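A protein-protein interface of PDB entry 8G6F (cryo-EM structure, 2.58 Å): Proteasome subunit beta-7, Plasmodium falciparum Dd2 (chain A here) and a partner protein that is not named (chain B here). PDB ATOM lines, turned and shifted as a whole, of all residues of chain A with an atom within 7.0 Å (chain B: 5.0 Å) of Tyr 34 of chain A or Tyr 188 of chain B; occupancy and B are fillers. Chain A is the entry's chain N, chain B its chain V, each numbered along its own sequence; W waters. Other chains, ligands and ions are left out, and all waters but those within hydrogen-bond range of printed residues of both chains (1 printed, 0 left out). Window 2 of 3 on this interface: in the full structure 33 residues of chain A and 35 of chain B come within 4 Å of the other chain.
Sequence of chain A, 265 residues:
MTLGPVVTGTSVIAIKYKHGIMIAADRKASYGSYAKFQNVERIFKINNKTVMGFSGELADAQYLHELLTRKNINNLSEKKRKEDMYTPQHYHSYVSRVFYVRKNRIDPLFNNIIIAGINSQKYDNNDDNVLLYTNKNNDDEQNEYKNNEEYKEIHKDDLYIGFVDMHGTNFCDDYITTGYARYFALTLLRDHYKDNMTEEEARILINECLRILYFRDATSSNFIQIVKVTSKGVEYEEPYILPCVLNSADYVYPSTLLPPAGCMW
Tyr 188 of chain B touches just one residue of chain A: Tyr 34.
Printed residues of chain A within 4 Å of Asn 222 of chain B: Lys 28 (2.8 Å), Ser 30 (3.1 Å), Gly 32 (3.5 Å), Ser 33 (2.8 Å) and Ala 35 (3.7 Å).
Of the printed residues of chain B, Gly 32 of chain A touches Asn 222 (3.5 Å).
Printed residues of chain B within 4 Å of Ala 35 of chain A: Asn 220 and Asn 222.
Of the printed residues of chain A, Asn 220 of chain B touches Tyr 34 (3.5 Å) and Ala 35 (3.2 Å).
The nearest residue of chain B that does not touch Tyr 34 of chain A is Asn 222 of chain B (4.2 Å).
The nearest residue of chain A that does not touch Tyr 188 of chain B is Ser 33 of chain A (4.2 Å).
Water W1 lies within hydrogen-bond range of OD1 of Asn 222 of chain B (3.0 Å), NZ of Lys 28 of chain A (3.4 Å) and O of Asp 221 of chain B (3.4 Å).
The side-chain amide oxygen (OD1) of Asn 222 of chain B lies within hydrogen-bond range of the side-chain amino group (NZ) of Lys 28 of chain A (2.8 Å).
ND2 of Asn 222 of chain B is in hydrogen-bond range of OG of Ser 30 of chain A (3.1 Å).
The backbone NH (N) of Asn 222 of chain B is in hydrogen-bond range of the backbone carbonyl oxygen (O) of Ser 33 of chain A, at 2.8 Å.
The backbone NH of Ala 35 of chain A is in hydrogen-bond range of the backbone carbonyl oxygen of Asn 220 of chain B, 3.2 Å away.
OD1 of Asp 221 of chain B sits close to O of Ser 33 of chain A (3.5 Å).
Gly 32 of chain A touches Asn 222 of chain B (O to ND2, 3.5 Å).
OH of Tyr 188 of chain B touches CB of Tyr 34 of chain A, at 3.3 Å.
Tyr 34 of chain A touches Asn 220 of chain B.
CB of Ala 35 of chain A touches OD1 of Asn 222 of chain B, 3.7 Å away.
Hydrophobic or aromatic side chains of chain B that line the printed part of chain A: Tyr 188.
Printed residues of chain A that touch a printed residue of chain B: Lys 28, Ser 30, Gly 32, Ser 33, Tyr 34 and Ala 35.
Hydrophobic or aromatic side chains of chain A within 4 Å of the printed part of chain B: Tyr 34 and Ala 35.
Among the printed residues, 9 pairs touch across the chains.
Among the printed residues, no Asp or Glu carboxylate lies within 4 Å of a Lys or Arg side-chain nitrogen of the other chain.
O of Ala 35 of chain A lies close to NE2 of Gln 38 of chain A, at 3.2 Å.
OG of Ser 184 of chain B is in hydrogen-bond range of OD2 of Asp 221 of chain B (3.0 Å).
The backbone NH (N) of Gly 185 of chain B sits at hydrogen-bond distance from the side-chain carboxylate (OD2) of Asp 221 of chain B, 3.4 Å away.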
ATOM      1  N   LYS A  28     -19.599  -2.412 -31.840  1.00  0.00           N
ATOM      2  CA  LYS A  28     -19.234  -3.307 -30.751  1.00  0.00           C
ATOM      3  C   LYS A  28     -17.888  -3.949 -31.038  1.00  0.00           C
ATOM      4  O   LYS A  28     -17.642  -4.409 -32.155  1.00  0.00           O
ATOM      5  CB  LYS A  28     -20.305  -4.385 -30.551  1.00  0.00           C
ATOM      6  CG  LYS A  28     -19.860  -5.564 -29.717  1.00  0.00           C
ATOM      7  CD  LYS A  28     -21.049  -6.358 -29.224  1.00  0.00           C
ATOM      8  CE  LYS A  28     -20.786  -7.844 -29.249  1.00  0.00           C
ATOM      9  NZ  LYS A  28     -21.967  -8.613 -28.792  1.00  0.00           N
ATOM     10  N   ALA A  29     -17.024  -3.972 -30.027  1.00  0.00           N
ATOM     11  CA  ALA A  29     -15.751  -4.674 -30.076  1.00  0.00           C
ATOM     12  C   ALA A  29     -15.700  -5.653 -28.915  1.00  0.00           C
ATOM     13  O   ALA A  29     -15.950  -5.272 -27.769  1.00  0.00           O
ATOM     14  CB  ALA A  29     -14.575  -3.697 -30.008  1.00  0.00           C
ATOM     15  N   SER A  30     -15.382  -6.907 -29.208  1.00  0.00           N
ATOM     16  CA  SER A  30     -15.457  -7.985 -28.234  1.00  0.00           C
ATOM     17  C   SER A  30     -14.060  -8.432 -27.840  1.00  0.00           C
ATOM     18  O   SER A  30     -13.204  -8.648 -28.700  1.00  0.00           O
ATOM     19  CB  SER A  30     -16.241  -9.175 -28.790  1.00  0.00           C
ATOM     20  OG  SER A  30     -17.579  -8.820 -29.076  1.00  0.00           O
ATOM     21  N   TYR A  31     -13.842  -8.573 -26.539  1.00  0.00           N
ATOM     22  CA  TYR A  31     -12.611  -9.149 -26.008  1.00  0.00           C
ATOM     23  C   TYR A  31     -12.849 -10.631 -25.723  1.00  0.00           C
ATOM     24  O   TYR A  31     -12.909 -11.083 -24.583  1.00  0.00           O
ATOM     25  CB  TYR A  31     -12.171  -8.380 -24.765  1.00  0.00           C
ATOM     26  CG  TYR A  31     -10.942  -8.913 -24.066  1.00  0.00           C
ATOM     27  CD1 TYR A  31     -10.090  -9.814 -24.684  1.00  0.00           C
ATOM     28  CD2 TYR A  31     -10.640  -8.514 -22.774  1.00  0.00           C
ATOM     29  CE1 TYR A  31      -8.974 -10.299 -24.036  1.00  0.00           C
ATOM     30  CE2 TYR A  31      -9.527  -8.993 -22.119  1.00  0.00           C
ATOM     31  CZ  TYR A  31      -8.696  -9.883 -22.753  1.00  0.00           C
ATOM     32  OH  TYR A  31      -7.586 -10.360 -22.100  1.00  0.00           O
ATOM     33  N   GLY A  32     -12.983 -11.381 -26.798  1.00  0.00           N
ATOM     34  CA  GLY A  32     -13.308 -12.802 -26.715  1.00  0.00           C
ATOM     35  C   GLY A  32     -14.813 -13.020 -26.798  1.00  0.00           C
ATOM     36  O   GLY A  32     -15.441 -12.615 -27.768  1.00  0.00           O
ATOM     37  N   SER A  33     -15.374 -13.670 -25.782  1.00  0.00           N
ATOM     38  CA  SER A  33     -16.816 -13.740 -25.607  1.00  0.00           C
ATOM     39  C   SER A  33     -17.342 -12.602 -24.751  1.00  0.00           C
ATOM     40  O   SER A  33     -18.541 -12.556 -24.469  1.00  0.00           O
ATOM     41  CB  SER A  33     -17.211 -15.075 -24.979  1.00  0.00           C
ATOM     42  OG  SER A  33     -16.580 -15.250 -23.725  1.00  0.00           O
ATOM     43  N   TYR A  34     -16.475 -11.688 -24.339  1.00  0.00           N
ATOM     44  CA  TYR A  34     -16.841 -10.579 -23.476  1.00  0.00           C
ATOM     45  C   TYR A  34     -17.036  -9.335 -24.331  1.00  0.00           C
ATOM     46  O   TYR A  34     -16.088  -8.852 -24.957  1.00  0.00           O
ATOM     47  CB  TYR A  34     -15.761 -10.363 -22.418  1.00  0.00           C
ATOM     48  CG  TYR A  34     -15.965  -9.164 -21.529  1.00  0.00           C
ATOM     49  CD1 TYR A  34     -17.235  -8.691 -21.242  1.00  0.00           C
ATOM     50  CD2 TYR A  34     -14.884  -8.515 -20.965  1.00  0.00           C
ATOM     51  CE1 TYR A  34     -17.416  -7.601 -20.429  1.00  0.00           C
ATOM     52  CE2 TYR A  34     -15.056  -7.427 -20.151  1.00  0.00           C
ATOM     53  CZ  TYR A  34     -16.322  -6.973 -19.887  1.00  0.00           C
ATOM     54  OH  TYR A  34     -16.486  -5.881 -19.072  1.00  0.00           O
ATOM     55  N   ALA A  35     -18.265  -8.824 -24.363  1.00  0.00           N
ATOM     56  CA  ALA A  35     -18.577  -7.606 -25.104  1.00  0.00           C
ATOM     57  C   ALA A  35     -18.159  -6.418 -24.248  1.00  0.00           C
ATOM     58  O   ALA A  35     -18.964  -5.774 -23.574  1.00  0.00           O
ATOM     59  CB  ALA A  35     -20.055  -7.556 -25.458  1.00  0.00           C
ATOM     60  N   LYS A  36     -16.859  -6.129 -24.276  1.00  0.00           N
ATOM     61  CA  LYS A  36     -16.317  -5.095 -23.404  1.00  0.00           C
ATOM     62  C   LYS A  36     -16.668  -3.692 -23.888  1.00  0.00           C
ATOM     63  O   LYS A  36     -16.982  -2.819 -23.074  1.00  0.00           O
ATOM     64  CB  LYS A  36     -14.802  -5.251 -23.289  1.00  0.00           C
ATOM     65  CG  LYS A  36     -14.204  -4.452 -22.149  1.00  0.00           C
ATOM     66  CD  LYS A  36     -12.756  -4.810 -21.900  1.00  0.00           C
ATOM     67  CE  LYS A  36     -12.196  -4.019 -20.734  1.00  0.00           C
ATOM     68  NZ  LYS A  36     -10.909  -4.574 -20.246  1.00  0.00           N
ATOM     69  N   PHE A  37     -16.618  -3.453 -25.195  1.00  0.00           N
ATOM     70  CA  PHE A  37     -16.851  -2.132 -25.761  1.00  0.00           C
ATOM     71  C   PHE A  37     -18.086  -2.170 -26.646  1.00  0.00           C
ATOM     72  O   PHE A  37     -18.169  -2.986 -27.565  1.00  0.00           O
ATOM     73  CB  PHE A  37     -15.636  -1.664 -26.559  1.00  0.00           C
ATOM     74  CG  PHE A  37     -14.355  -1.745 -25.793  1.00  0.00           C
ATOM     75  CD1 PHE A  37     -14.064  -0.822 -24.809  1.00  0.00           C
ATOM     76  CD2 PHE A  37     -13.450  -2.754 -26.041  1.00  0.00           C
ATOM     77  CE1 PHE A  37     -12.895  -0.902 -24.099  1.00  0.00           C
ATOM     78  CE2 PHE A  37     -12.282  -2.835 -25.330  1.00  0.00           C
ATOM     79  CZ  PHE A  37     -12.005  -1.909 -24.360  1.00  0.00           C
ATOM     80  N   GLN A  38     -19.039  -1.282 -26.367  1.00  0.00           N
ATOM     81  CA  GLN A  38     -20.322  -1.283 -27.047  1.00  0.00           C
ATOM     82  C   GLN A  38     -20.575  -0.026 -27.863  1.00  0.00           C
ATOM     83  O   GLN A  38     -21.651   0.094 -28.457  1.00  0.00           O
ATOM     84  CB  GLN A  38     -21.465  -1.447 -26.037  1.00  0.00           C
ATOM     85  CG  GLN A  38     -21.315  -2.608 -25.067  1.00  0.00           C
ATOM     86  CD  GLN A  38     -22.123  -3.824 -25.460  1.00  0.00           C
ATOM     87  OE1 GLN A  38     -23.130  -3.720 -26.154  1.00  0.00           O
ATOM     88  NE2 GLN A  38     -21.705  -4.984 -24.985  1.00  0.00           N
ATOM     89  N   SER B 184     -21.237 -19.035 -18.483  1.00  0.00           N
ATOM     90  CA  SER B 184     -20.240 -18.005 -18.740  1.00  0.00           C
ATOM     91  C   SER B 184     -20.741 -16.621 -18.352  1.00  0.00           C
ATOM     92  O   SER B 184     -19.943 -15.764 -17.963  1.00  0.00           O
ATOM     93  CB  SER B 184     -19.842 -18.027 -20.213  1.00  0.00           C
ATOM     94  OG  SER B 184     -20.974 -18.215 -21.038  1.00  0.00           O
ATOM     95  N   GLY B 185     -22.050 -16.382 -18.448  1.00  0.00           N
ATOM     96  CA  GLY B 185     -22.584 -15.061 -18.178  1.00  0.00           C
ATOM     97  C   GLY B 185     -22.759 -14.735 -16.714  1.00  0.00           C
ATOM     98  O   GLY B 185     -22.909 -13.560 -16.369  1.00  0.00           O
ATOM     99  N   SER B 186     -22.747 -15.746 -15.844  1.00  0.00           N
ATOM    100  CA  SER B 186     -22.955 -15.505 -14.420  1.00  0.00           C
ATOM    101  C   SER B 186     -21.832 -14.676 -13.815  1.00  0.00           C
ATOM    102  O   SER B 186     -22.050 -13.953 -12.831  1.00  0.00           O
ATOM    103  CB  SER B 186     -23.077 -16.836 -13.687  1.00  0.00           C
ATOM    104  OG  SER B 186     -21.949 -17.656 -13.928  1.00  0.00           O
ATOM    105  N   ILE B 187     -20.631 -14.769 -14.380  1.00  0.00           N
ATOM    106  CA  ILE B 187     -19.497 -14.037 -13.830  1.00  0.00           C
ATOM    107  C   ILE B 187     -19.785 -12.544 -13.836  1.00  0.00           C
ATOM    108  O   ILE B 187     -19.459 -11.831 -12.883  1.00  0.00           O
ATOM    109  CB  ILE B 187     -18.214 -14.367 -14.616  1.00  0.00           C
ATOM    110  CG1 ILE B 187     -17.985 -15.882 -14.675  1.00  0.00           C
ATOM    111  CG2 ILE B 187     -17.016 -13.691 -13.984  1.00  0.00           C
ATOM    112  CD1 ILE B 187     -17.660 -16.521 -13.340  1.00  0.00           C
ATOM    113  N   TYR B 188     -20.414 -12.052 -14.903  1.00  0.00           N
ATOM    114  CA  TYR B 188     -20.649 -10.622 -15.041  1.00  0.00           C
ATOM    115  C   TYR B 188     -21.662 -10.096 -14.036  1.00  0.00           C
ATOM    116  O   TYR B 188     -21.630  -8.905 -13.714  1.00  0.00           O
ATOM    117  CB  TYR B 188     -21.112 -10.312 -16.462  1.00  0.00           C
ATOM    118  CG  TYR B 188     -20.166 -10.822 -17.522  1.00  0.00           C
ATOM    119  CD1 TYR B 188     -18.916 -10.253 -17.698  1.00  0.00           C
ATOM    120  CD2 TYR B 188     -20.520 -11.876 -18.341  1.00  0.00           C
ATOM    121  CE1 TYR B 188     -18.055 -10.719 -18.656  1.00  0.00           C
ATOM    122  CE2 TYR B 188     -19.667 -12.346 -19.300  1.00  0.00           C
ATOM    123  CZ  TYR B 188     -18.435 -11.766 -19.456  1.00  0.00           C
ATOM    124  OH  TYR B 188     -17.579 -12.241 -20.418  1.00  0.00           O
ATOM    125  N   ILE B 189     -22.549 -10.948 -13.529  1.00  0.00           N
ATOM    126  CA  ILE B 189     -23.580 -10.542 -12.581  1.00  0.00           C
ATOM    127  C   ILE B 189     -23.289 -11.013 -11.173  1.00  0.00           C
ATOM    128  O   ILE B 189     -24.134 -10.831 -10.288  1.00  0.00           O
ATOM    129  CB  ILE B 189     -24.969 -11.039 -13.020  1.00  0.00           C
ATOM    130  CG1 ILE B 189     -24.928 -12.539 -13.314  1.00  0.00           C
ATOM    131  CG2 ILE B 189     -25.445 -10.266 -14.225  1.00  0.00           C
ATOM    132  CD1 ILE B 189     -26.160 -13.277 -12.887  1.00  0.00           C
ATOM    133  N   GLN B 190     -22.133 -11.633 -10.935  1.00  0.00           N
ATOM    134  CA  GLN B 190     -21.802 -12.113  -9.598  1.00  0.00           C
ATOM    135  C   GLN B 190     -22.030 -11.044  -8.531  1.00  0.00           C
ATOM    136  O   GLN B 190     -22.822 -11.236  -7.604  1.00  0.00           O
ATOM    137  CB  GLN B 190     -20.350 -12.595  -9.572  1.00  0.00           C
ATOM    138  CG  GLN B 190     -20.005 -13.483  -8.394  1.00  0.00           C
ATOM    139  CD  GLN B 190     -21.046 -14.551  -8.147  1.00  0.00           C
ATOM    140  OE1 GLN B 190     -21.465 -15.245  -9.069  1.00  0.00           O
ATOM    141  NE2 GLN B 190     -21.473 -14.687  -6.900  1.00  0.00           N
ATOM    142  N   ALA B 217     -26.474 -10.365 -17.656  1.00  0.00           N
ATOM    143  CA  ALA B 217     -25.578 -11.394 -18.163  1.00  0.00           C
ATOM    144  C   ALA B 217     -25.622 -11.456 -19.681  1.00  0.00           C
ATOM    145  O   ALA B 217     -24.581 -11.582 -20.334  1.00  0.00           O
ATOM    146  CB  ALA B 217     -25.939 -12.746 -17.559  1.00  0.00           C
ATOM    147  N   ASN B 220     -23.750  -8.489 -21.267  1.00  0.00           N
ATOM    148  CA  ASN B 220     -22.295  -8.489 -21.187  1.00  0.00           C
ATOM    149  C   ASN B 220     -21.636  -9.706 -21.822  1.00  0.00           C
ATOM    150  O   ASN B 220     -20.440  -9.650 -22.121  1.00  0.00           O
ATOM    151  CB  ASN B 220     -21.854  -8.397 -19.727  1.00  0.00           C
ATOM    152  CG  ASN B 220     -22.052  -7.021 -19.151  1.00  0.00           C
ATOM    153  OD1 ASN B 220     -22.844  -6.830 -18.234  1.00  0.00           O
ATOM    154  ND2 ASN B 220     -21.335  -6.049 -19.690  1.00  0.00           N
ATOM    155  N   ASP B 221     -22.368 -10.792 -22.043  1.00  0.00           N
ATOM    156  CA  ASP B 221     -21.795 -12.054 -22.490  1.00  0.00           C
ATOM    157  C   ASP B 221     -22.259 -12.367 -23.905  1.00  0.00           C
ATOM    158  O   ASP B 221     -23.458 -12.324 -24.193  1.00  0.00           O
ATOM    159  CB  ASP B 221     -22.194 -13.186 -21.540  1.00  0.00           C
ATOM    160  CG  ASP B 221     -21.416 -14.463 -21.784  1.00  0.00           C
ATOM    161  OD1 ASP B 221     -20.192 -14.395 -22.008  1.00  0.00           O
ATOM    162  OD2 ASP B 221     -22.031 -15.543 -21.741  1.00  0.00           O
ATOM    163  N   ASN B 222     -21.306 -12.681 -24.784  1.00  0.00           N
ATOM    164  CA  ASN B 222     -21.636 -13.019 -26.162  1.00  0.00           C
ATOM    165  C   ASN B 222     -22.283 -14.389 -26.280  1.00  0.00           C
ATOM    166  O   ASN B 222     -23.003 -14.639 -27.251  1.00  0.00           O
ATOM    167  CB  ASN B 222     -20.381 -12.985 -27.032  1.00  0.00           C
ATOM    168  CG  ASN B 222     -19.990 -11.589 -27.438  1.00  0.00           C
ATOM    169  OD1 ASN B 222     -20.793 -10.663 -27.375  1.00  0.00           O
ATOM    170  ND2 ASN B 222     -18.749 -11.428 -27.864  1.00  0.00           N
HETATM  171  O   HOH W   1     -22.704  -9.243 -25.549  1.00  0.00           O
